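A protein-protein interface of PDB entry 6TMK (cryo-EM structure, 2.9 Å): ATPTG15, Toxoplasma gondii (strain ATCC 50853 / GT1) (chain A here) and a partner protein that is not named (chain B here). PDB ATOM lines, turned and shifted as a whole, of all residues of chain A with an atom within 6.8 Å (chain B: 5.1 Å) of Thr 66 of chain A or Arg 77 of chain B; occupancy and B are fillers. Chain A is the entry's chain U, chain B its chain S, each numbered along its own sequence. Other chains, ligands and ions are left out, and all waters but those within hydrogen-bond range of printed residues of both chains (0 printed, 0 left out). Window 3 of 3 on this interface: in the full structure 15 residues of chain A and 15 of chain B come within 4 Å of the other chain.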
ATOM      1  N   ARG A  61     -22.363 -18.938  -0.672  1.00  0.00           N
ATOM      2  CA  ARG A  61     -21.591 -19.018  -1.906  1.00  0.00           C
ATOM      3  C   ARG A  61     -21.871 -17.845  -2.831  1.00  0.00           C
ATOM      4  O   ARG A  61     -20.961 -17.380  -3.523  1.00  0.00           O
ATOM      5  CB  ARG A  61     -21.888 -20.325  -2.629  1.00  0.00           C
ATOM      6  CG  ARG A  61     -21.583 -21.566  -1.835  1.00  0.00           C
ATOM      7  CD  ARG A  61     -20.128 -21.612  -1.436  1.00  0.00           C
ATOM      8  NE  ARG A  61     -19.257 -21.581  -2.604  1.00  0.00           N
ATOM      9  CZ  ARG A  61     -17.949 -21.794  -2.560  1.00  0.00           C
ATOM     10  NH1 ARG A  61     -17.358 -22.055  -1.408  1.00  0.00           N
ATOM     11  NH2 ARG A  61     -17.233 -21.747  -3.669  1.00  0.00           N
ATOM     12  N   ALA A  62     -23.104 -17.346  -2.857  1.00  0.00           N
ATOM     13  CA  ALA A  62     -23.415 -16.191  -3.686  1.00  0.00           C
ATOM     14  C   ALA A  62     -22.590 -14.989  -3.263  1.00  0.00           C
ATOM     15  O   ALA A  62     -21.938 -14.341  -4.091  1.00  0.00           O
ATOM     16  CB  ALA A  62     -24.904 -15.876  -3.600  1.00  0.00           C
ATOM     17  N   MET A  63     -22.606 -14.673  -1.969  1.00  0.00           N
ATOM     18  CA  MET A  63     -21.863 -13.517  -1.490  1.00  0.00           C
ATOM     19  C   MET A  63     -20.367 -13.714  -1.696  1.00  0.00           C
ATOM     20  O   MET A  63     -19.655 -12.780  -2.096  1.00  0.00           O
ATOM     21  CB  MET A  63     -22.202 -13.278  -0.021  1.00  0.00           C
ATOM     22  CG  MET A  63     -21.886 -11.893   0.491  1.00  0.00           C
ATOM     23  SD  MET A  63     -22.839 -11.489   1.968  1.00  0.00           S
ATOM     24  CE  MET A  63     -22.154 -12.627   3.163  1.00  0.00           C
ATOM     25  N   ARG A  64     -19.879 -14.934  -1.470  1.00  0.00           N
ATOM     26  CA  ARG A  64     -18.465 -15.214  -1.681  1.00  0.00           C
ATOM     27  C   ARG A  64     -18.064 -14.971  -3.130  1.00  0.00           C
ATOM     28  O   ARG A  64     -17.068 -14.292  -3.404  1.00  0.00           O
ATOM     29  CB  ARG A  64     -18.153 -16.649  -1.270  1.00  0.00           C
ATOM     30  CG  ARG A  64     -16.796 -17.126  -1.696  1.00  0.00           C
ATOM     31  CD  ARG A  64     -16.293 -18.219  -0.794  1.00  0.00           C
ATOM     32  NE  ARG A  64     -15.049 -18.794  -1.291  1.00  0.00           N
ATOM     33  CZ  ARG A  64     -14.225 -19.530  -0.560  1.00  0.00           C
ATOM     34  NH1 ARG A  64     -14.505 -19.784   0.707  1.00  0.00           N
ATOM     35  NH2 ARG A  64     -13.120 -20.013  -1.099  1.00  0.00           N
ATOM     36  N   LEU A  65     -18.820 -15.530  -4.074  1.00  0.00           N
ATOM     37  CA  LEU A  65     -18.466 -15.378  -5.476  1.00  0.00           C
ATOM     38  C   LEU A  65     -18.631 -13.944  -5.954  1.00  0.00           C
ATOM     39  O   LEU A  65     -17.912 -13.510  -6.860  1.00  0.00           O
ATOM     40  CB  LEU A  65     -19.338 -16.292  -6.329  1.00  0.00           C
ATOM     41  CG  LEU A  65     -19.192 -17.796  -6.124  1.00  0.00           C
ATOM     42  CD1 LEU A  65     -20.243 -18.514  -6.932  1.00  0.00           C
ATOM     43  CD2 LEU A  65     -17.813 -18.279  -6.490  1.00  0.00           C
ATOM     44  N   THR A  66     -19.563 -13.195  -5.368  1.00  0.00           N
ATOM     45  CA  THR A  66     -19.804 -11.842  -5.846  1.00  0.00           C
ATOM     46  C   THR A  66     -18.795 -10.841  -5.299  1.00  0.00           C
ATOM     47  O   THR A  66     -18.504  -9.844  -5.969  1.00  0.00           O
ATOM     48  CB  THR A  66     -21.221 -11.400  -5.494  1.00  0.00           C
ATOM     49  OG1 THR A  66     -22.138 -12.469  -5.749  1.00  0.00           O
ATOM     50  CG2 THR A  66     -21.616 -10.214  -6.335  1.00  0.00           C
ATOM     51  N   PHE A  67     -18.255 -11.072  -4.099  1.00  0.00           N
ATOM     52  CA  PHE A  67     -17.397 -10.085  -3.456  1.00  0.00           C
ATOM     53  C   PHE A  67     -16.061 -10.613  -2.956  1.00  0.00           C
ATOM     54  O   PHE A  67     -15.193  -9.800  -2.624  1.00  0.00           O
ATOM     55  CB  PHE A  67     -18.124  -9.428  -2.277  1.00  0.00           C
ATOM     56  CG  PHE A  67     -19.483  -8.912  -2.618  1.00  0.00           C
ATOM     57  CD1 PHE A  67     -19.650  -7.985  -3.628  1.00  0.00           C
ATOM     58  CD2 PHE A  67     -20.593  -9.348  -1.929  1.00  0.00           C
ATOM     59  CE1 PHE A  67     -20.900  -7.510  -3.945  1.00  0.00           C
ATOM     60  CE2 PHE A  67     -21.844  -8.875  -2.242  1.00  0.00           C
ATOM     61  CZ  PHE A  67     -21.998  -7.956  -3.250  1.00  0.00           C
ATOM     62  N   PHE A  68     -15.861 -11.923  -2.893  1.00  0.00           N
ATOM     63  CA  PHE A  68     -14.703 -12.505  -2.226  1.00  0.00           C
ATOM     64  C   PHE A  68     -14.094 -13.616  -3.070  1.00  0.00           C
ATOM     65  O   PHE A  68     -13.853 -14.726  -2.595  1.00  0.00           O
ATOM     66  CB  PHE A  68     -15.084 -13.034  -0.849  1.00  0.00           C
ATOM     67  CG  PHE A  68     -15.594 -11.983   0.082  1.00  0.00           C
ATOM     68  CD1 PHE A  68     -16.948 -11.829   0.297  1.00  0.00           C
ATOM     69  CD2 PHE A  68     -14.720 -11.151   0.746  1.00  0.00           C
ATOM     70  CE1 PHE A  68     -17.418 -10.863   1.153  1.00  0.00           C
ATOM     71  CE2 PHE A  68     -15.185 -10.185   1.603  1.00  0.00           C
ATOM     72  CZ  PHE A  68     -16.535 -10.040   1.806  1.00  0.00           C
ATOM     73  N   ASP A  69     -13.832 -13.332  -4.344  1.00  0.00           N
ATOM     74  CA  ASP A  69     -13.179 -14.320  -5.194  1.00  0.00           C
ATOM     75  C   ASP A  69     -12.338 -13.638  -6.261  1.00  0.00           C
ATOM     76  O   ASP A  69     -12.844 -12.827  -7.041  1.00  0.00           O
ATOM     77  CB  ASP A  69     -14.223 -15.225  -5.847  1.00  0.00           C
ATOM     78  CG  ASP A  69     -13.656 -16.560  -6.271  1.00  0.00           C
ATOM     79  OD1 ASP A  69     -12.435 -16.638  -6.517  1.00  0.00           O
ATOM     80  OD2 ASP A  69     -14.430 -17.534  -6.360  1.00  0.00           O
ATOM     81  N   VAL A  73     -10.937 -15.838 -11.591  1.00  0.00           N
ATOM     82  CA  VAL A  73     -10.318 -15.058 -12.657  1.00  0.00           C
ATOM     83  C   VAL A  73      -8.902 -15.548 -12.913  1.00  0.00           C
ATOM     84  O   VAL A  73      -8.483 -15.734 -14.065  1.00  0.00           O
ATOM     85  CB  VAL A  73     -10.338 -13.563 -12.294  1.00  0.00           C
ATOM     86  CG1 VAL A  73      -9.422 -12.774 -13.196  1.00  0.00           C
ATOM     87  CG2 VAL A  73     -11.736 -13.037 -12.374  1.00  0.00           C
ATOM     88  N   ALA B  72     -10.166  -5.906  -4.892  1.00  0.00           N
ATOM     89  CA  ALA B  72      -9.416  -6.770  -5.788  1.00  0.00           C
ATOM     90  C   ALA B  72     -10.336  -7.589  -6.675  1.00  0.00           C
ATOM     91  O   ALA B  72     -10.016  -7.835  -7.836  1.00  0.00           O
ATOM     92  CB  ALA B  72      -8.510  -7.685  -4.978  1.00  0.00           C
ATOM     93  N   SER B  73     -11.470  -8.043  -6.145  1.00  0.00           N
ATOM     94  CA  SER B  73     -12.415  -8.785  -6.968  1.00  0.00           C
ATOM     95  C   SER B  73     -12.925  -7.926  -8.114  1.00  0.00           C
ATOM     96  O   SER B  73     -12.955  -8.362  -9.274  1.00  0.00           O
ATOM     97  CB  SER B  73     -13.571  -9.272  -6.105  1.00  0.00           C
ATOM     98  OG  SER B  73     -13.099 -10.060  -5.036  1.00  0.00           O
ATOM     99  N   CYS B  74     -13.319  -6.688  -7.809  1.00  0.00           N
ATOM    100  CA  CYS B  74     -13.766  -5.786  -8.869  1.00  0.00           C
ATOM    101  C   CYS B  74     -12.666  -5.570  -9.905  1.00  0.00           C
ATOM    102  O   CYS B  74     -12.896  -5.675 -11.125  1.00  0.00           O
ATOM    103  CB  CYS B  74     -14.208  -4.463  -8.255  1.00  0.00           C
ATOM    104  SG  CYS B  74     -15.733  -4.574  -7.304  1.00  0.00           S
ATOM    105  N   ARG B  75     -11.457  -5.266  -9.431  1.00  0.00           N
ATOM    106  CA  ARG B  75     -10.344  -5.005 -10.334  1.00  0.00           C
ATOM    107  C   ARG B  75     -10.035  -6.218 -11.197  1.00  0.00           C
ATOM    108  O   ARG B  75      -9.766  -6.082 -12.394  1.00  0.00           O
ATOM    109  CB  ARG B  75      -9.121  -4.579  -9.525  1.00  0.00           C
ATOM    110  CG  ARG B  75      -7.832  -4.459 -10.312  1.00  0.00           C
ATOM    111  CD  ARG B  75      -7.961  -3.493 -11.462  1.00  0.00           C
ATOM    112  NE  ARG B  75      -8.289  -2.148 -11.010  1.00  0.00           N
ATOM    113  CZ  ARG B  75      -8.867  -1.227 -11.771  1.00  0.00           C
ATOM    114  NH1 ARG B  75      -9.185  -1.498 -13.025  1.00  0.00           N
ATOM    115  NH2 ARG B  75      -9.128  -0.033 -11.273  1.00  0.00           N
ATOM    116  N   TYR B  76     -10.066  -7.411 -10.608  1.00  0.00           N
ATOM    117  CA  TYR B  76      -9.736  -8.620 -11.346  1.00  0.00           C
ATOM    118  C   TYR B  76     -10.786  -8.920 -12.400  1.00  0.00           C
ATOM    119  O   TYR B  76     -10.461  -9.404 -13.486  1.00  0.00           O
ATOM    120  CB  TYR B  76      -9.609  -9.792 -10.380  1.00  0.00           C
ATOM    121  CG  TYR B  76      -8.234  -9.970  -9.793  1.00  0.00           C
ATOM    122  CD1 TYR B  76      -7.568 -11.176  -9.889  1.00  0.00           C
ATOM    123  CD2 TYR B  76      -7.606  -8.932  -9.139  1.00  0.00           C
ATOM    124  CE1 TYR B  76      -6.316 -11.338  -9.354  1.00  0.00           C
ATOM    125  CE2 TYR B  76      -6.359  -9.086  -8.600  1.00  0.00           C
ATOM    126  CZ  TYR B  76      -5.717 -10.289  -8.705  1.00  0.00           C
ATOM    127  OH  TYR B  76      -4.464 -10.443  -8.172  1.00  0.00           O
ATOM    128  N   ARG B  77     -12.054  -8.650 -12.094  1.00  0.00           N
ATOM    129  CA  ARG B  77     -13.100  -8.806 -13.098  1.00  0.00           C
ATOM    130  C   ARG B  77     -12.834  -7.908 -14.303  1.00  0.00           C
ATOM    131  O   ARG B  77     -12.819  -8.367 -15.461  1.00  0.00           O
ATOM    132  CB  ARG B  77     -14.450  -8.492 -12.465  1.00  0.00           C
ATOM    133  CG  ARG B  77     -15.601  -9.266 -13.027  1.00  0.00           C
ATOM    134  CD  ARG B  77     -16.855  -9.026 -12.228  1.00  0.00           C
ATOM    135  NE  ARG B  77     -16.873  -9.851 -11.021  1.00  0.00           N
ATOM    136  CZ  ARG B  77     -16.966  -9.389  -9.775  1.00  0.00           C
ATOM    137  NH1 ARG B  77     -17.054  -8.092  -9.524  1.00  0.00           N
ATOM    138  NH2 ARG B  77     -16.963 -10.242  -8.766  1.00  0.00           N
ATOM    139  N   LYS B  78     -12.621  -6.614 -14.046  1.00  0.00           N
ATOM    140  CA  LYS B  78     -12.331  -5.694 -15.143  1.00  0.00           C
ATOM    141  C   LYS B  78     -11.099  -6.132 -15.923  1.00  0.00           C
ATOM    142  O   LYS B  78     -11.069  -6.057 -17.159  1.00  0.00           O
ATOM    143  CB  LYS B  78     -12.137  -4.280 -14.607  1.00  0.00           C
ATOM    144  CG  LYS B  78     -13.370  -3.670 -13.994  1.00  0.00           C
ATOM    145  CD  LYS B  78     -13.062  -2.288 -13.457  1.00  0.00           C
ATOM    146  CE  LYS B  78     -14.032  -1.865 -12.371  1.00  0.00           C
ATOM    147  NZ  LYS B  78     -13.451  -0.789 -11.519  1.00  0.00           N
ATOM    148  N   LEU B  79     -10.075  -6.593 -15.212  1.00  0.00           N
ATOM    149  CA  LEU B  79      -8.827  -6.981 -15.850  1.00  0.00           C
ATOM    150  C   LEU B  79      -9.013  -8.209 -16.725  1.00  0.00           C
ATOM    151  O   LEU B  79      -8.408  -8.308 -17.795  1.00  0.00           O
ATOM    152  CB  LEU B  79      -7.771  -7.226 -14.781  1.00  0.00           C
ATOM    153  CG  LEU B  79      -6.432  -7.773 -15.237  1.00  0.00           C
ATOM    154  CD1 LEU B  79      -5.708  -6.781 -16.103  1.00  0.00           C
ATOM    155  CD2 LEU B  79      -5.633  -8.089 -14.017  1.00  0.00           C
ATOM    156  N   ASN B  80      -9.819  -9.167 -16.276  1.00  0.00           N
ATOM    157  CA  ASN B  80     -10.096 -10.346 -17.081  1.00  0.00           C
ATOM    158  C   ASN B  80     -10.783  -9.955 -18.381  1.00  0.00           C
ATOM    159  O   ASN B  80     -10.421 -10.433 -19.467  1.00  0.00           O
ATOM    160  CB  ASN B  80     -10.964 -11.304 -16.272  1.00  0.00           C
ATOM    161  CG  ASN B  80     -11.073 -12.666 -16.896  1.00  0.00           C
ATOM    162  OD1 ASN B  80     -10.078 -13.271 -17.287  1.00  0.00           O
ATOM    163  ND2 ASN B  80     -12.292 -13.163 -16.987  1.00  0.00           N
ATOM    164  N   GLU B  81     -11.780  -9.072 -18.286  1.00  0.00           N
ATOM    165  CA  GLU B  81     -12.438  -8.569 -19.489  1.00  0.00           C
ATOM    166  C   GLU B  81     -11.430  -7.944 -20.449  1.00  0.00           C
ATOM    167  O   GLU B  81     -11.385  -8.280 -21.646  1.00  0.00           O
ATOM    168  CB  GLU B  81     -13.511  -7.558 -19.100  1.00  0.00           C
ATOM    169  CG  GLU B  81     -14.401  -7.126 -20.231  1.00  0.00           C
ATOM    170  CD  GLU B  81     -15.650  -6.422 -19.747  1.00  0.00           C
ATOM    171  OE1 GLU B  81     -16.518  -7.093 -19.151  1.00  0.00           O
ATOM    172  OE2 GLU B  81     -15.763  -5.197 -19.957  1.00  0.00           O
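N of Asp 69 of chain A sits at hydrogen-bond distance from OG of Ser 73 of chain B, 3.4 Å away. NH2 of Arg 77 of chain B lies within hydrogen-bond range of O of Thr 66 of chain A (3.2 Å). The side-chain hydroxyl (OG) of Ser 73 of chain B lies within hydrogen-bond range of the backbone carbonyl oxygen (O) of Phe 67 of chain A.
Hydrophobic or aromatic side chains of chain A that line the printed part of chain B: Val 73. Among the printed residues, no Asp or Glu carboxylate lies within 4 Å of a Lys or Arg side-chain nitrogen of the other chain.
Among the printed residues, pairs that only touch across the chains: Val 73 of chain A with Tyr 76 of chain B (3.5 Å), Val 73 of chain A with Asn 80 of chain B (3.7 Å), Leu 65 of chain A with Arg 77 of chain B (3.9 Å) and Phe 68 of chain A with Ser 73 of chain B (3.96 Å).
O of Ala 62 of chain A lies within hydrogen-bond range of OG1 of Thr 66 of chain A (2.5 Å).
Thr 66 of chain A touches one residue of chain B. Arg 77 of chain B touches just these residues of chain A: Leu 65 (3.9 Å) and Thr 66 (3.2 Å). Of the printed residues of chain B, Val 73 of chain A touches Tyr 76 (3.5 Å) and Asn 80 (3.7 Å). Of the printed residues of chain A, Ser 73 of chain B touches Phe 67, Phe 68 and Asp 69. Printed residues of chain A within 4 Å of Asn 80 of chain B: Val 73 (3.7 Å). Glu 81 of chain B touches none of the printed residues of chain A. Lys 78 of chain B touches none of the printed residues of chain A.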
